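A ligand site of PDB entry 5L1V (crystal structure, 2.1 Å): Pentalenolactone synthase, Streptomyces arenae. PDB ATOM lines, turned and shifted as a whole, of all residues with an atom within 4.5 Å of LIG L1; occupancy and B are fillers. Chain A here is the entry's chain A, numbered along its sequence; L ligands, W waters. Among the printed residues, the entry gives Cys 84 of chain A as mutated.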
ATOM      1  N   CYS A  84      -0.644   3.273 -16.386  1.00  0.00           N
ATOM      2  CA  CYS A  84       0.606   2.520 -16.253  1.00  0.00           C
ATOM      3  C   CYS A  84       1.108   1.993 -17.595  1.00  0.00           C
ATOM      4  O   CYS A  84       2.024   1.164 -17.610  1.00  0.00           O
ATOM      5  CB  CYS A  84       0.418   1.345 -15.275  1.00  0.00           C
ATOM      6  SG  CYS A  84       0.210   1.793 -13.499  1.00  0.00           S
ATOM      7  N   HIS A  96       5.948   1.421 -21.862  1.00  0.00           N
ATOM      8  CA  HIS A  96       6.328   1.429 -20.450  1.00  0.00           C
ATOM      9  C   HIS A  96       7.786   1.841 -20.264  1.00  0.00           C
ATOM     10  O   HIS A  96       8.106   2.543 -19.299  1.00  0.00           O
ATOM     11  CB  HIS A  96       6.049   0.075 -19.816  1.00  0.00           C
ATOM     12  CG  HIS A  96       6.591  -0.042 -18.421  1.00  0.00           C
ATOM     13  ND1 HIS A  96       5.987   0.564 -17.335  1.00  0.00           N
ATOM     14  CD2 HIS A  96       7.630  -0.741 -17.924  1.00  0.00           C
ATOM     15  CE1 HIS A  96       6.667   0.284 -16.244  1.00  0.00           C
ATOM     16  NE2 HIS A  96       7.670  -0.511 -16.575  1.00  0.00           N
ATOM     17  N   MET A  99       7.701   5.538 -20.493  1.00  0.00           N
ATOM     18  CA  MET A  99       7.126   6.072 -19.267  1.00  0.00           C
ATOM     19  C   MET A  99       8.156   6.227 -18.171  1.00  0.00           C
ATOM     20  O   MET A  99       8.273   7.291 -17.541  1.00  0.00           O
ATOM     21  CB  MET A  99       5.993   5.182 -18.764  1.00  0.00           C
ATOM     22  CG  MET A  99       5.192   5.852 -17.658  1.00  0.00           C
ATOM     23  SD  MET A  99       3.875   4.786 -17.096  1.00  0.00           S
ATOM     24  CE  MET A  99       4.005   4.807 -15.324  1.00  0.00           C
ATOM     25  N   ARG A 100       8.900   5.150 -17.903  1.00  0.00           N
ATOM     26  CA  ARG A 100       9.896   5.192 -16.836  1.00  0.00           C
ATOM     27  C   ARG A 100      11.053   6.111 -17.192  1.00  0.00           C
ATOM     28  O   ARG A 100      11.578   6.822 -16.323  1.00  0.00           O
ATOM     29  CB  ARG A 100      10.360   3.777 -16.519  1.00  0.00           C
ATOM     30  CG  ARG A 100       9.228   2.968 -15.873  1.00  0.00           C
ATOM     31  CD  ARG A 100       9.712   1.717 -15.210  1.00  0.00           C
ATOM     32  NE  ARG A 100      10.622   1.929 -14.072  1.00  0.00           N
ATOM     33  CZ  ARG A 100      10.260   2.038 -12.804  1.00  0.00           C
ATOM     34  NH1 ARG A 100       8.982   1.966 -12.428  1.00  0.00           N
ATOM     35  NH2 ARG A 100      11.195   2.191 -11.874  1.00  0.00           N
ATOM     36  N   LEU A 103       9.808   9.706 -16.483  1.00  0.00           N
ATOM     37  CA  LEU A 103       9.453  10.092 -15.113  1.00  0.00           C
ATOM     38  C   LEU A 103      10.630  10.024 -14.131  1.00  0.00           C
ATOM     39  O   LEU A 103      10.719  10.868 -13.221  1.00  0.00           O
ATOM     40  CB  LEU A 103       8.301   9.198 -14.600  1.00  0.00           C
ATOM     41  CG  LEU A 103       6.900   9.407 -15.203  1.00  0.00           C
ATOM     42  CD1 LEU A 103       5.911   8.399 -14.637  1.00  0.00           C
ATOM     43  CD2 LEU A 103       6.367  10.808 -14.990  1.00  0.00           C
ATOM     44  N   PHE A 107      12.599  13.097 -10.612  1.00  0.00           N
ATOM     45  CA  PHE A 107      12.812  12.995  -9.177  1.00  0.00           C
ATOM     46  C   PHE A 107      14.311  13.025  -8.886  1.00  0.00           C
ATOM     47  O   PHE A 107      14.845  12.140  -8.220  1.00  0.00           O
ATOM     48  CB  PHE A 107      12.144  11.732  -8.632  1.00  0.00           C
ATOM     49  CG  PHE A 107      10.632  11.716  -8.839  1.00  0.00           C
ATOM     50  CD1 PHE A 107      10.083  11.277 -10.047  1.00  0.00           C
ATOM     51  CD2 PHE A 107       9.768  12.143  -7.839  1.00  0.00           C
ATOM     52  CE1 PHE A 107       8.705  11.262 -10.249  1.00  0.00           C
ATOM     53  CE2 PHE A 107       8.395  12.135  -8.036  1.00  0.00           C
ATOM     54  CZ  PHE A 107       7.857  11.695  -9.234  1.00  0.00           C
ATOM     55  N   LEU A 155       5.225  19.405  -7.094  1.00  0.00           N
ATOM     56  CA  LEU A 155       5.719  18.732  -8.292  1.00  0.00           C
ATOM     57  C   LEU A 155       5.082  19.303  -9.546  1.00  0.00           C
ATOM     58  O   LEU A 155       5.750  19.442 -10.581  1.00  0.00           O
ATOM     59  CB  LEU A 155       5.438  17.228  -8.202  1.00  0.00           C
ATOM     60  CG  LEU A 155       6.123  16.375  -7.136  1.00  0.00           C
ATOM     61  CD1 LEU A 155       5.430  15.004  -7.080  1.00  0.00           C
ATOM     62  CD2 LEU A 155       7.606  16.218  -7.426  1.00  0.00           C
ATOM     63  N   PHE A 235      -1.304   8.850  -8.706  1.00  0.00           N
ATOM     64  CA  PHE A 235      -0.487   7.946  -7.884  1.00  0.00           C
ATOM     65  C   PHE A 235       0.333   8.674  -6.838  1.00  0.00           C
ATOM     66  O   PHE A 235       0.863   8.034  -5.919  1.00  0.00           O
ATOM     67  CB  PHE A 235       0.470   7.124  -8.781  1.00  0.00           C
ATOM     68  CG  PHE A 235      -0.212   6.329  -9.877  1.00  0.00           C
ATOM     69  CD1 PHE A 235       0.502   5.951 -11.005  1.00  0.00           C
ATOM     70  CD2 PHE A 235      -1.560   5.940  -9.772  1.00  0.00           C
ATOM     71  CE1 PHE A 235      -0.096   5.222 -12.043  1.00  0.00           C
ATOM     72  CE2 PHE A 235      -2.165   5.190 -10.813  1.00  0.00           C
ATOM     73  CZ  PHE A 235      -1.424   4.837 -11.948  1.00  0.00           C
ATOM     74  N   GLY A 236       0.459  10.008  -6.939  1.00  0.00           N
ATOM     75  CA  GLY A 236       1.435  10.731  -6.149  1.00  0.00           C
ATOM     76  C   GLY A 236       1.008  11.224  -4.784  1.00  0.00           C
ATOM     77  O   GLY A 236       1.850  11.729  -4.048  1.00  0.00           O
ATOM     78  N   THR A 239      -1.781   7.181  -1.899  1.00  0.00           N
ATOM     79  CA  THR A 239      -1.180   6.073  -1.158  1.00  0.00           C
ATOM     80  C   THR A 239      -0.282   6.570  -0.038  1.00  0.00           C
ATOM     81  O   THR A 239      -0.145   5.893   0.993  1.00  0.00           O
ATOM     82  CB  THR A 239      -0.389   5.144  -2.102  1.00  0.00           C
ATOM     83  OG1 THR A 239       0.578   5.893  -2.845  1.00  0.00           O
ATOM     84  CG2 THR A 239      -1.313   4.377  -3.045  1.00  0.00           C
ATOM     85  N   THR A 240       0.353   7.741  -0.203  1.00  0.00           N
ATOM     86  CA  THR A 240       1.125   8.322   0.905  1.00  0.00           C
ATOM     87  C   THR A 240       0.219   8.721   2.067  1.00  0.00           C
ATOM     88  O   THR A 240       0.562   8.487   3.227  1.00  0.00           O
ATOM     89  CB  THR A 240       1.926   9.539   0.415  1.00  0.00           C
ATOM     90  OG1 THR A 240       2.630   9.194  -0.772  1.00  0.00           O
ATOM     91  CG2 THR A 240       2.924   9.957   1.463  1.00  0.00           C
ATOM     92  N   ARG A 243      -0.463   5.718   4.028  1.00  0.00           N
ATOM     93  CA  ARG A 243       0.651   5.248   4.858  1.00  0.00           C
ATOM     94  C   ARG A 243       0.850   6.117   6.101  1.00  0.00           C
ATOM     95  O   ARG A 243       1.290   5.608   7.134  1.00  0.00           O
ATOM     96  CB  ARG A 243       1.949   5.194   4.027  1.00  0.00           C
ATOM     97  CG  ARG A 243       1.945   4.094   2.932  1.00  0.00           C
ATOM     98  CD  ARG A 243       1.006   2.935   3.332  1.00  0.00           C
ATOM     99  NE  ARG A 243       0.944   1.828   2.365  1.00  0.00           N
ATOM    100  CZ  ARG A 243       0.170   1.813   1.288  1.00  0.00           C
ATOM    101  NH1 ARG A 243      -0.603   2.855   0.997  1.00  0.00           N
ATOM    102  NH2 ARG A 243       0.149   0.728   0.500  1.00  0.00           N
ATOM    103  N   LEU A 276       6.027   0.874   6.451  1.00  0.00           N
ATOM    104  CA  LEU A 276       5.757   0.409   5.084  1.00  0.00           C
ATOM    105  C   LEU A 276       5.597  -1.109   5.041  1.00  0.00           C
ATOM    106  O   LEU A 276       4.723  -1.629   4.347  1.00  0.00           O
ATOM    107  CB  LEU A 276       6.899   0.856   4.156  1.00  0.00           C
ATOM    108  CG  LEU A 276       6.997   2.361   3.899  1.00  0.00           C
ATOM    109  CD1 LEU A 276       8.382   2.749   3.306  1.00  0.00           C
ATOM    110  CD2 LEU A 276       5.873   2.820   2.989  1.00  0.00           C
ATOM    111  N   ILE A 289      -0.206  -7.066  -6.010  1.00  0.00           N
ATOM    112  CA  ILE A 289       0.246  -6.551  -7.295  1.00  0.00           C
ATOM    113  C   ILE A 289      -0.225  -7.517  -8.379  1.00  0.00           C
ATOM    114  O   ILE A 289       0.183  -8.690  -8.357  1.00  0.00           O
ATOM    115  CB  ILE A 289       1.770  -6.376  -7.344  1.00  0.00           C
ATOM    116  CG1 ILE A 289       2.210  -5.245  -6.404  1.00  0.00           C
ATOM    117  CG2 ILE A 289       2.239  -6.116  -8.796  1.00  0.00           C
ATOM    118  CD1 ILE A 289       3.729  -4.988  -6.416  1.00  0.00           C
ATOM    119  N   ARG A 291      -0.720  -9.377 -12.061  1.00  0.00           N
ATOM    120  CA  ARG A 291       0.076  -9.682 -13.249  1.00  0.00           C
ATOM    121  C   ARG A 291      -0.640 -10.726 -14.080  1.00  0.00           C
ATOM    122  O   ARG A 291      -1.570 -11.397 -13.612  1.00  0.00           O
ATOM    123  CB  ARG A 291       1.472 -10.203 -12.853  1.00  0.00           C
ATOM    124  CG  ARG A 291       2.380  -9.200 -12.136  1.00  0.00           C
ATOM    125  CD  ARG A 291       2.660  -7.978 -13.016  1.00  0.00           C
ATOM    126  NE  ARG A 291       3.712  -7.149 -12.439  1.00  0.00           N
ATOM    127  CZ  ARG A 291       3.528  -5.917 -11.992  1.00  0.00           C
ATOM    128  NH1 ARG A 291       2.321  -5.362 -12.036  1.00  0.00           N
ATOM    129  NH2 ARG A 291       4.546  -5.225 -11.497  1.00  0.00           N
ATOM    130  N   ILE A 314       2.332  -8.675  -1.870  1.00  0.00           N
ATOM    131  CA  ILE A 314       3.446  -7.963  -1.239  1.00  0.00           C
ATOM    132  C   ILE A 314       3.178  -7.756   0.248  1.00  0.00           C
ATOM    133  O   ILE A 314       4.112  -7.775   1.064  1.00  0.00           O
ATOM    134  CB  ILE A 314       3.712  -6.622  -1.969  1.00  0.00           C
ATOM    135  CG1 ILE A 314       2.450  -5.747  -2.007  1.00  0.00           C
ATOM    136  CG2 ILE A 314       4.233  -6.863  -3.370  1.00  0.00           C
ATOM    137  CD1 ILE A 314       2.679  -4.329  -2.588  1.00  0.00           C
ATOM    138  N   ALA A 342       6.905  -3.267  -0.206  1.00  0.00           N
ATOM    139  CA  ALA A 342       5.738  -2.373  -0.239  1.00  0.00           C
ATOM    140  C   ALA A 342       5.769  -1.364  -1.386  1.00  0.00           C
ATOM    141  O   ALA A 342       4.712  -0.793  -1.709  1.00  0.00           O
ATOM    142  CB  ALA A 342       5.608  -1.615   1.079  1.00  0.00           C
ATOM    143  N   PHE A 343       6.929  -1.080  -1.958  1.00  0.00           N
ATOM    144  CA  PHE A 343       7.054  -0.300  -3.187  1.00  0.00           C
ATOM    145  C   PHE A 343       7.211  -1.191  -4.426  1.00  0.00           C
ATOM    146  O   PHE A 343       7.567  -0.688  -5.506  1.00  0.00           O
ATOM    147  CB  PHE A 343       8.259   0.637  -3.100  1.00  0.00           C
ATOM    148  CG  PHE A 343       8.122   1.745  -2.104  1.00  0.00           C
ATOM    149  CD1 PHE A 343       7.044   2.629  -2.146  1.00  0.00           C
ATOM    150  CD2 PHE A 343       9.103   1.952  -1.137  1.00  0.00           C
ATOM    151  CE1 PHE A 343       6.953   3.683  -1.237  1.00  0.00           C
ATOM    152  CE2 PHE A 343       9.020   2.992  -0.218  1.00  0.00           C
ATOM    153  CZ  PHE A 343       7.931   3.862  -0.268  1.00  0.00           C
ATOM    154  N   GLY A 344       7.003  -2.499  -4.283  1.00  0.00           N
ATOM    155  CA  GLY A 344       7.247  -3.424  -5.360  1.00  0.00           C
ATOM    156  C   GLY A 344       8.732  -3.698  -5.585  1.00  0.00           C
ATOM    157  O   GLY A 344       9.583  -3.518  -4.700  1.00  0.00           O
ATOM    158  N   ALA A 347      10.690  -4.363 -12.725  1.00  0.00           N
ATOM    159  CA  ALA A 347      10.479  -3.404 -13.822  1.00  0.00           C
ATOM    160  C   ALA A 347       9.555  -2.237 -13.447  1.00  0.00           C
ATOM    161  O   ALA A 347       9.686  -1.134 -14.000  1.00  0.00           O
ATOM    162  CB  ALA A 347       9.924  -4.108 -15.062  1.00  0.00           C
ATOM    163  N   ARG A 348       8.613  -2.434 -12.531  1.00  0.00           N
ATOM    164  CA  ARG A 348       7.689  -1.355 -12.198  1.00  0.00           C
ATOM    165  C   ARG A 348       7.863  -0.841 -10.764  1.00  0.00           C
ATOM    166  O   ARG A 348       6.943  -0.225 -10.221  1.00  0.00           O
ATOM    167  CB  ARG A 348       6.227  -1.785 -12.441  1.00  0.00           C
ATOM    168  CG  ARG A 348       5.932  -2.204 -13.912  1.00  0.00           C
ATOM    169  CD  ARG A 348       4.470  -2.661 -14.135  1.00  0.00           C
ATOM    170  NE  ARG A 348       4.110  -2.686 -15.567  1.00  0.00           N
ATOM    171  CZ  ARG A 348       3.663  -1.624 -16.234  1.00  0.00           C
ATOM    172  NH1 ARG A 348       3.526  -0.457 -15.616  1.00  0.00           N
ATOM    173  NH2 ARG A 348       3.355  -1.701 -17.520  1.00  0.00           N
ATOM    174  N   HIS A 349       9.037  -1.042 -10.175  1.00  0.00           N
ATOM    175  CA  HIS A 349       9.412  -0.472  -8.878  1.00  0.00           C
ATOM    176  C   HIS A 349       8.979   0.990  -8.775  1.00  0.00           C
ATOM    177  O   HIS A 349       9.283   1.803  -9.661  1.00  0.00           O
ATOM    178  CB  HIS A 349      10.941  -0.595  -8.702  1.00  0.00           C
ATOM    179  CG  HIS A 349      11.411  -0.660  -7.273  1.00  0.00           C
ATOM    180  ND1 HIS A 349      12.732  -0.830  -6.940  1.00  0.00           N
ATOM    181  CD2 HIS A 349      10.728  -0.560  -6.095  1.00  0.00           C
ATOM    182  CE1 HIS A 349      12.854  -0.844  -5.611  1.00  0.00           C
ATOM    183  NE2 HIS A 349      11.655  -0.672  -5.085  1.00  0.00           N
ATOM    184  N   CYS A 350       8.234   1.302  -7.708  1.00  0.00           N
ATOM    185  CA  CYS A 350       7.677   2.625  -7.435  1.00  0.00           C
ATOM    186  C   CYS A 350       8.646   3.755  -7.786  1.00  0.00           C
ATOM    187  O   CYS A 350       9.754   3.843  -7.240  1.00  0.00           O
ATOM    188  CB  CYS A 350       7.289   2.730  -5.951  1.00  0.00           C
ATOM    189  SG  CYS A 350       6.760   4.416  -5.513  1.00  0.00           S
ATOM    190  N   ILE A 351       8.204   4.660  -8.662  1.00  0.00           N
ATOM    191  CA  ILE A 351       9.053   5.763  -9.085  1.00  0.00           C
ATOM    192  C   ILE A 351       9.173   6.829  -7.997  1.00  0.00           C
ATOM    193  O   ILE A 351      10.208   7.480  -7.860  1.00  0.00           O
ATOM    194  CB  ILE A 351       8.524   6.339 -10.417  1.00  0.00           C
ATOM    195  CG1 ILE A 351       8.976   5.451 -11.592  1.00  0.00           C
ATOM    196  CG2 ILE A 351       8.976   7.766 -10.650  1.00  0.00           C
ATOM    197  CD1 ILE A 351       8.070   5.505 -12.784  1.00  0.00           C
ATOM    198  N   GLY A 352       8.120   7.013  -7.186  1.00  0.00           N
ATOM    199  CA  GLY A 352       8.126   8.031  -6.146  1.00  0.00           C
ATOM    200  C   GLY A 352       8.660   7.612  -4.793  1.00  0.00           C
ATOM    201  O   GLY A 352       8.551   8.372  -3.838  1.00  0.00           O
ATOM    202  N   LEU A 355      10.856   9.962  -2.657  1.00  0.00           N
ATOM    203  CA  LEU A 355      10.088  11.106  -2.179  1.00  0.00           C
ATOM    204  C   LEU A 355       9.078  10.691  -1.111  1.00  0.00           C
ATOM    205  O   LEU A 355       8.890  11.411  -0.128  1.00  0.00           O
ATOM    206  CB  LEU A 355       9.386  11.781  -3.374  1.00  0.00           C
ATOM    207  CG  LEU A 355       8.437  12.929  -3.006  1.00  0.00           C
ATOM    208  CD1 LEU A 355       9.187  14.060  -2.326  1.00  0.00           C
ATOM    209  CD2 LEU A 355       7.709  13.454  -4.230  1.00  0.00           C
ATOM    210  N   ALA A 356       8.403   9.557  -1.305  1.00  0.00           N
ATOM    211  CA  ALA A 356       7.460   9.089  -0.288  1.00  0.00           C
ATOM    212  C   ALA A 356       8.160   8.837   1.045  1.00  0.00           C
ATOM    213  O   ALA A 356       7.636   9.184   2.113  1.00  0.00           O
ATOM    214  CB  ALA A 356       6.752   7.810  -0.774  1.00  0.00           C
ATOM    215  N   LEU A 360       7.331  10.539   4.717  1.00  0.00           N
ATOM    216  CA  LEU A 360       7.036   9.731   5.895  1.00  0.00           C
ATOM    217  C   LEU A 360       8.054   9.973   7.006  1.00  0.00           C
ATOM    218  O   LEU A 360       7.685  10.041   8.190  1.00  0.00           O
ATOM    219  CB  LEU A 360       6.953   8.259   5.508  1.00  0.00           C
ATOM    220  CG  LEU A 360       5.781   7.819   4.604  1.00  0.00           C
ATOM    221  CD1 LEU A 360       5.831   6.325   4.283  1.00  0.00           C
ATOM    222  CD2 LEU A 360       4.388   8.172   5.191  1.00  0.00           C
HETATM  223  C1  LIG L   1       4.287   2.135  -8.731  1.00  0.00           C
HETATM  224  C2  LIG L   1       3.539   1.853  -3.947  1.00  0.00           C
HETATM  225  C3  LIG L   1       4.015   6.662  -3.538  1.00  0.00           C
HETATM  226  C4  LIG L   1       4.527   7.024  -8.342  1.00  0.00           C
HETATM  227  C5  LIG L   1       4.102   1.591  -7.473  1.00  0.00           C
HETATM  228  C6  LIG L   1       4.039   0.184  -7.098  1.00  0.00           C
HETATM  229  C7  LIG L   1       3.828   0.139  -5.768  1.00  0.00           C
HETATM  230  C8  LIG L   1       3.762   1.492  -5.254  1.00  0.00           C
HETATM  231  C9  LIG L   1       3.672  -1.131  -4.884  1.00  0.00           C
HETATM  232  C10 LIG L   1       4.215  -1.065  -8.018  1.00  0.00           C
HETATM  233  C11 LIG L   1       3.050  -1.304  -8.992  1.00  0.00           C
HETATM  234  C12 LIG L   1       3.307  -2.542  -9.833  1.00  0.00           C
HETATM  235  O1  LIG L   1       4.363  -3.217  -9.592  1.00  0.00           O
HETATM  236  O2  LIG L   1       2.471  -2.852 -10.738  1.00  0.00           O
HETATM  237  C13 LIG L   1       3.587   3.126  -3.391  1.00  0.00           C
HETATM  238  C14 LIG L   1       3.446   3.471  -1.986  1.00  0.00           C
HETATM  239  C15 LIG L   1       3.569   4.811  -1.893  1.00  0.00           C
HETATM  240  C16 LIG L   1       3.823   5.343  -3.221  1.00  0.00           C
HETATM  241  C17 LIG L   1       3.169   2.465  -0.842  1.00  0.00           C
HETATM  242  C18 LIG L   1       3.512   5.728  -0.643  1.00  0.00           C
HETATM  243  C19 LIG L   1       4.052   5.353   0.525  1.00  0.00           C
HETATM  244  C20 LIG L   1       4.232   7.189  -4.788  1.00  0.00           C
HETATM  245  C21 LIG L   1       4.553   8.569  -5.072  1.00  0.00           C
HETATM  246  C22 LIG L   1       4.695   8.677  -6.412  1.00  0.00           C
HETATM  247  C23 LIG L   1       4.478   7.363  -7.000  1.00  0.00           C
HETATM  248  C24 LIG L   1       4.693   9.657  -3.954  1.00  0.00           C
HETATM  249  C25 LIG L   1       5.007   9.918  -7.292  1.00  0.00           C
HETATM  250  C26 LIG L   1       4.967  11.177  -6.849  1.00  0.00           C
HETATM  251  C27 LIG L   1       4.445   5.750  -8.874  1.00  0.00           C
HETATM  252  C28 LIG L   1       4.355   5.393 -10.279  1.00  0.00           C
HETATM  253  C29 LIG L   1       4.286   4.054 -10.376  1.00  0.00           C
HETATM  254  C30 LIG L   1       4.322   3.493  -9.039  1.00  0.00           C
HETATM  255  C31 LIG L   1       4.354   6.396 -11.444  1.00  0.00           C
HETATM  256  C32 LIG L   1       4.187   3.221 -11.667  1.00  0.00           C
HETATM  257  C33 LIG L   1       5.510   2.520 -11.924  1.00  0.00           C
HETATM  258  C34 LIG L   1       5.472   1.677 -13.167  1.00  0.00           C
HETATM  259  O3  LIG L   1       6.557   1.586 -13.806  1.00  0.00           O
HETATM  260  O4  LIG L   1       4.396   1.094 -13.511  1.00  0.00           O
HETATM  261  N1  LIG L   1       3.950   2.354  -6.334  1.00  0.00           N
HETATM  262  N2  LIG L   1       3.827   4.285  -4.102  1.00  0.00           N
HETATM  263  N3  LIG L   1       4.198   6.485  -5.979  1.00  0.00           N
HETATM  264  N4  LIG L   1       4.411   4.556  -8.151  1.00  0.00           N
HETATM  265 FE1  LIG L   1       4.346   4.403  -6.090  1.00  0.00          FE
HETATM  266  C1  LG2 L   2       0.736   1.625  -6.804  1.00  0.00           C
HETATM  267  C2  LG2 L   2      -0.402   1.990  -7.754  1.00  0.00           C
HETATM  268  C3  LG2 L   2       0.159   2.381  -9.123  1.00  0.00           C
HETATM  269  C4  LG2 L   2      -1.232   3.167  -7.202  1.00  0.00           C
HETATM  270  C5  LG2 L   2      -0.028   0.600  -4.592  1.00  0.00           C
HETATM  271  C6  LG2 L   2      -3.159  -0.614  -5.252  1.00  0.00           C
HETATM  272  C7  LG2 L   2      -0.449  -2.581  -5.791  1.00  0.00           C
HETATM  273  C8  LG2 L   2      -1.184   0.656  -7.907  1.00  0.00           C
HETATM  274  C9  LG2 L   2      -1.841   0.881  -3.077  1.00  0.00           C
HETATM  275  C10 LG2 L   2      -2.509  -1.935  -7.150  1.00  0.00           C
HETATM  276  C11 LG2 L   2      -1.351   0.703  -4.334  1.00  0.00           C
HETATM  277  C12 LG2 L   2       0.256   0.370  -5.975  1.00  0.00           C
HETATM  278  C13 LG2 L   2      -2.107   0.515  -5.506  1.00  0.00           C
HETATM  279  C14 LG2 L   2      -1.216  -1.595  -6.691  1.00  0.00           C
HETATM  280  C15 LG2 L   2      -1.110  -0.041  -6.523  1.00  0.00           C
HETATM  281  O1  LG2 L   2      -1.095   0.909  -2.071  1.00  0.00           O
HETATM  282  O2  LG2 L   2      -2.668  -2.629  -8.156  1.00  0.00           O
HETATM  283  O3  LG2 L   2      -3.055   1.069  -2.866  1.00  0.00           O
HETATM  284  O4  LG2 L   2      -3.549  -1.368  -6.449  1.00  0.00           O
HETATM  285  O5  LG2 L   2      -0.084  -2.328  -7.189  1.00  0.00           O
HETATM  286  O   HOH W   1       1.863  -0.260 -12.192  1.00  0.00           O
HETATM  287  O   HOH W   2       1.164   8.580  -2.989  1.00  0.00           O
HETATM  288  O   HOH W   3       6.762  -3.411  -8.838  1.00  0.00           O
HETATM  289  O   HOH W   4      -0.462  -2.822 -10.191  1.00  0.00           O
HETATM  290  O   HOH W   5       1.204   5.226  -5.417  1.00  0.00           O
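Residues that only touch LIG L1: His 96 (2.8 Å), Thr 239 (3.3 Å), Ala 342 (3.4 Å), Arg 243 (3.4 Å), Gly 352 (3.5 Å), Gly 236 (3.5 Å), Phe 343 (3.6 Å), Thr 240 (3.6 Å), Gly 344 (3.7 Å), Phe 235 (3.7 Å), Ile 289 (3.7 Å), Phe 107 (3.8 Å), Ile 351 (3.8 Å), Ala 356 (3.9 Å), Leu 155 (3.9 Å), Leu 276 (3.98 Å) and Met 99 (3.99 Å). Hydrophobic or aromatic side chains that line LIG L1: His 96, Met 99, Phe 107, Leu 155, Phe 235, Leu 276, Ile 289, Phe 343 and Ala 356. Within 4 Å of LIG L1: His 96, Met 99, Arg 100, Phe 107, Leu 155, Phe 235, Gly 236, Thr 239, Thr 240, Arg 243, Leu 276, Ile 289, Arg 291, Ala 342, Phe 343, Gly 344, Arg 348, Cys 350, Ile 351, Gly 352 and Ala 356.
NH1 of Arg 348 sits at hydrogen-bond distance from O of Cys 84 (3.0 Å). The backbone NH of Gly 352 sits close to the side-chain sulfur of Cys 350. The guanidinium group of Arg 100 is in hydrogen-bond range of the backbone carbonyl oxygen of His 349, at 2.8 Å. The guanidinium group (NE) of Arg 100 lies close to the backbone carbonyl oxygen (O) of Ala 347. The backbone carbonyl oxygen of Ala 347 lies within hydrogen-bond range of a ring nitrogen (NE2) of His 96 (3.3 Å). The backbone carbonyl oxygen of Phe 343 sits at hydrogen-bond distance from the backbone NH of Cys 350. O of Thr 239 lies within hydrogen-bond range of NH1 of Arg 243 (3.1 Å). The guanidinium group of Arg 348 lies within hydrogen-bond range of a ring nitrogen (ND1) of His 96 (3.2 Å).
The side-chain sulfur (SG) of Cys 350 binds an iron atom (FE1) of LIG L1 (2.5 Å). The guanidinium group (NH1) of Arg 100 is in salt-bridge range of an oxygen (O3) of LIG L1 (2.8 Å). The guanidinium group of Arg 348 is in salt-bridge range of an oxygen (O4) of LIG L1, at 2.8 Å. An oxygen (O1) of LG2 L2 lies within salt-bridge range of the guanidinium group of Arg 243, 2.9 Å away. The guanidinium group (NH2) of Arg 291 lies within salt-bridge range of an oxygen (O1) of LIG L1 (2.8 Å).
Water W3 lies within hydrogen-bond range of an oxygen (O1) of LIG L1 (2.5 Å) and the backbone carbonyl oxygen of Arg 348 (3.5 Å). Water W4 lies within hydrogen-bond range of O2 of LIG L1 (3.0 Å) and O2 of LG2 L2 (3.0 Å). Water W1 bridges the side-chain sulfur (SG) of Cys 84 (2.9 Å) and an oxygen (O2) of LIG L1 (3.0 Å). Water W5 bridges OG1 of Thr 239 (2.7 Å) and O of Phe 235 (2.9 Å). Water W2 lies within hydrogen-bond range of OG1 of Thr 240 (2.7 Å), OG1 of Thr 239 (2.8 Å), O of Phe 235 (3.0 Å) and O of Gly 236 (3.4 Å).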
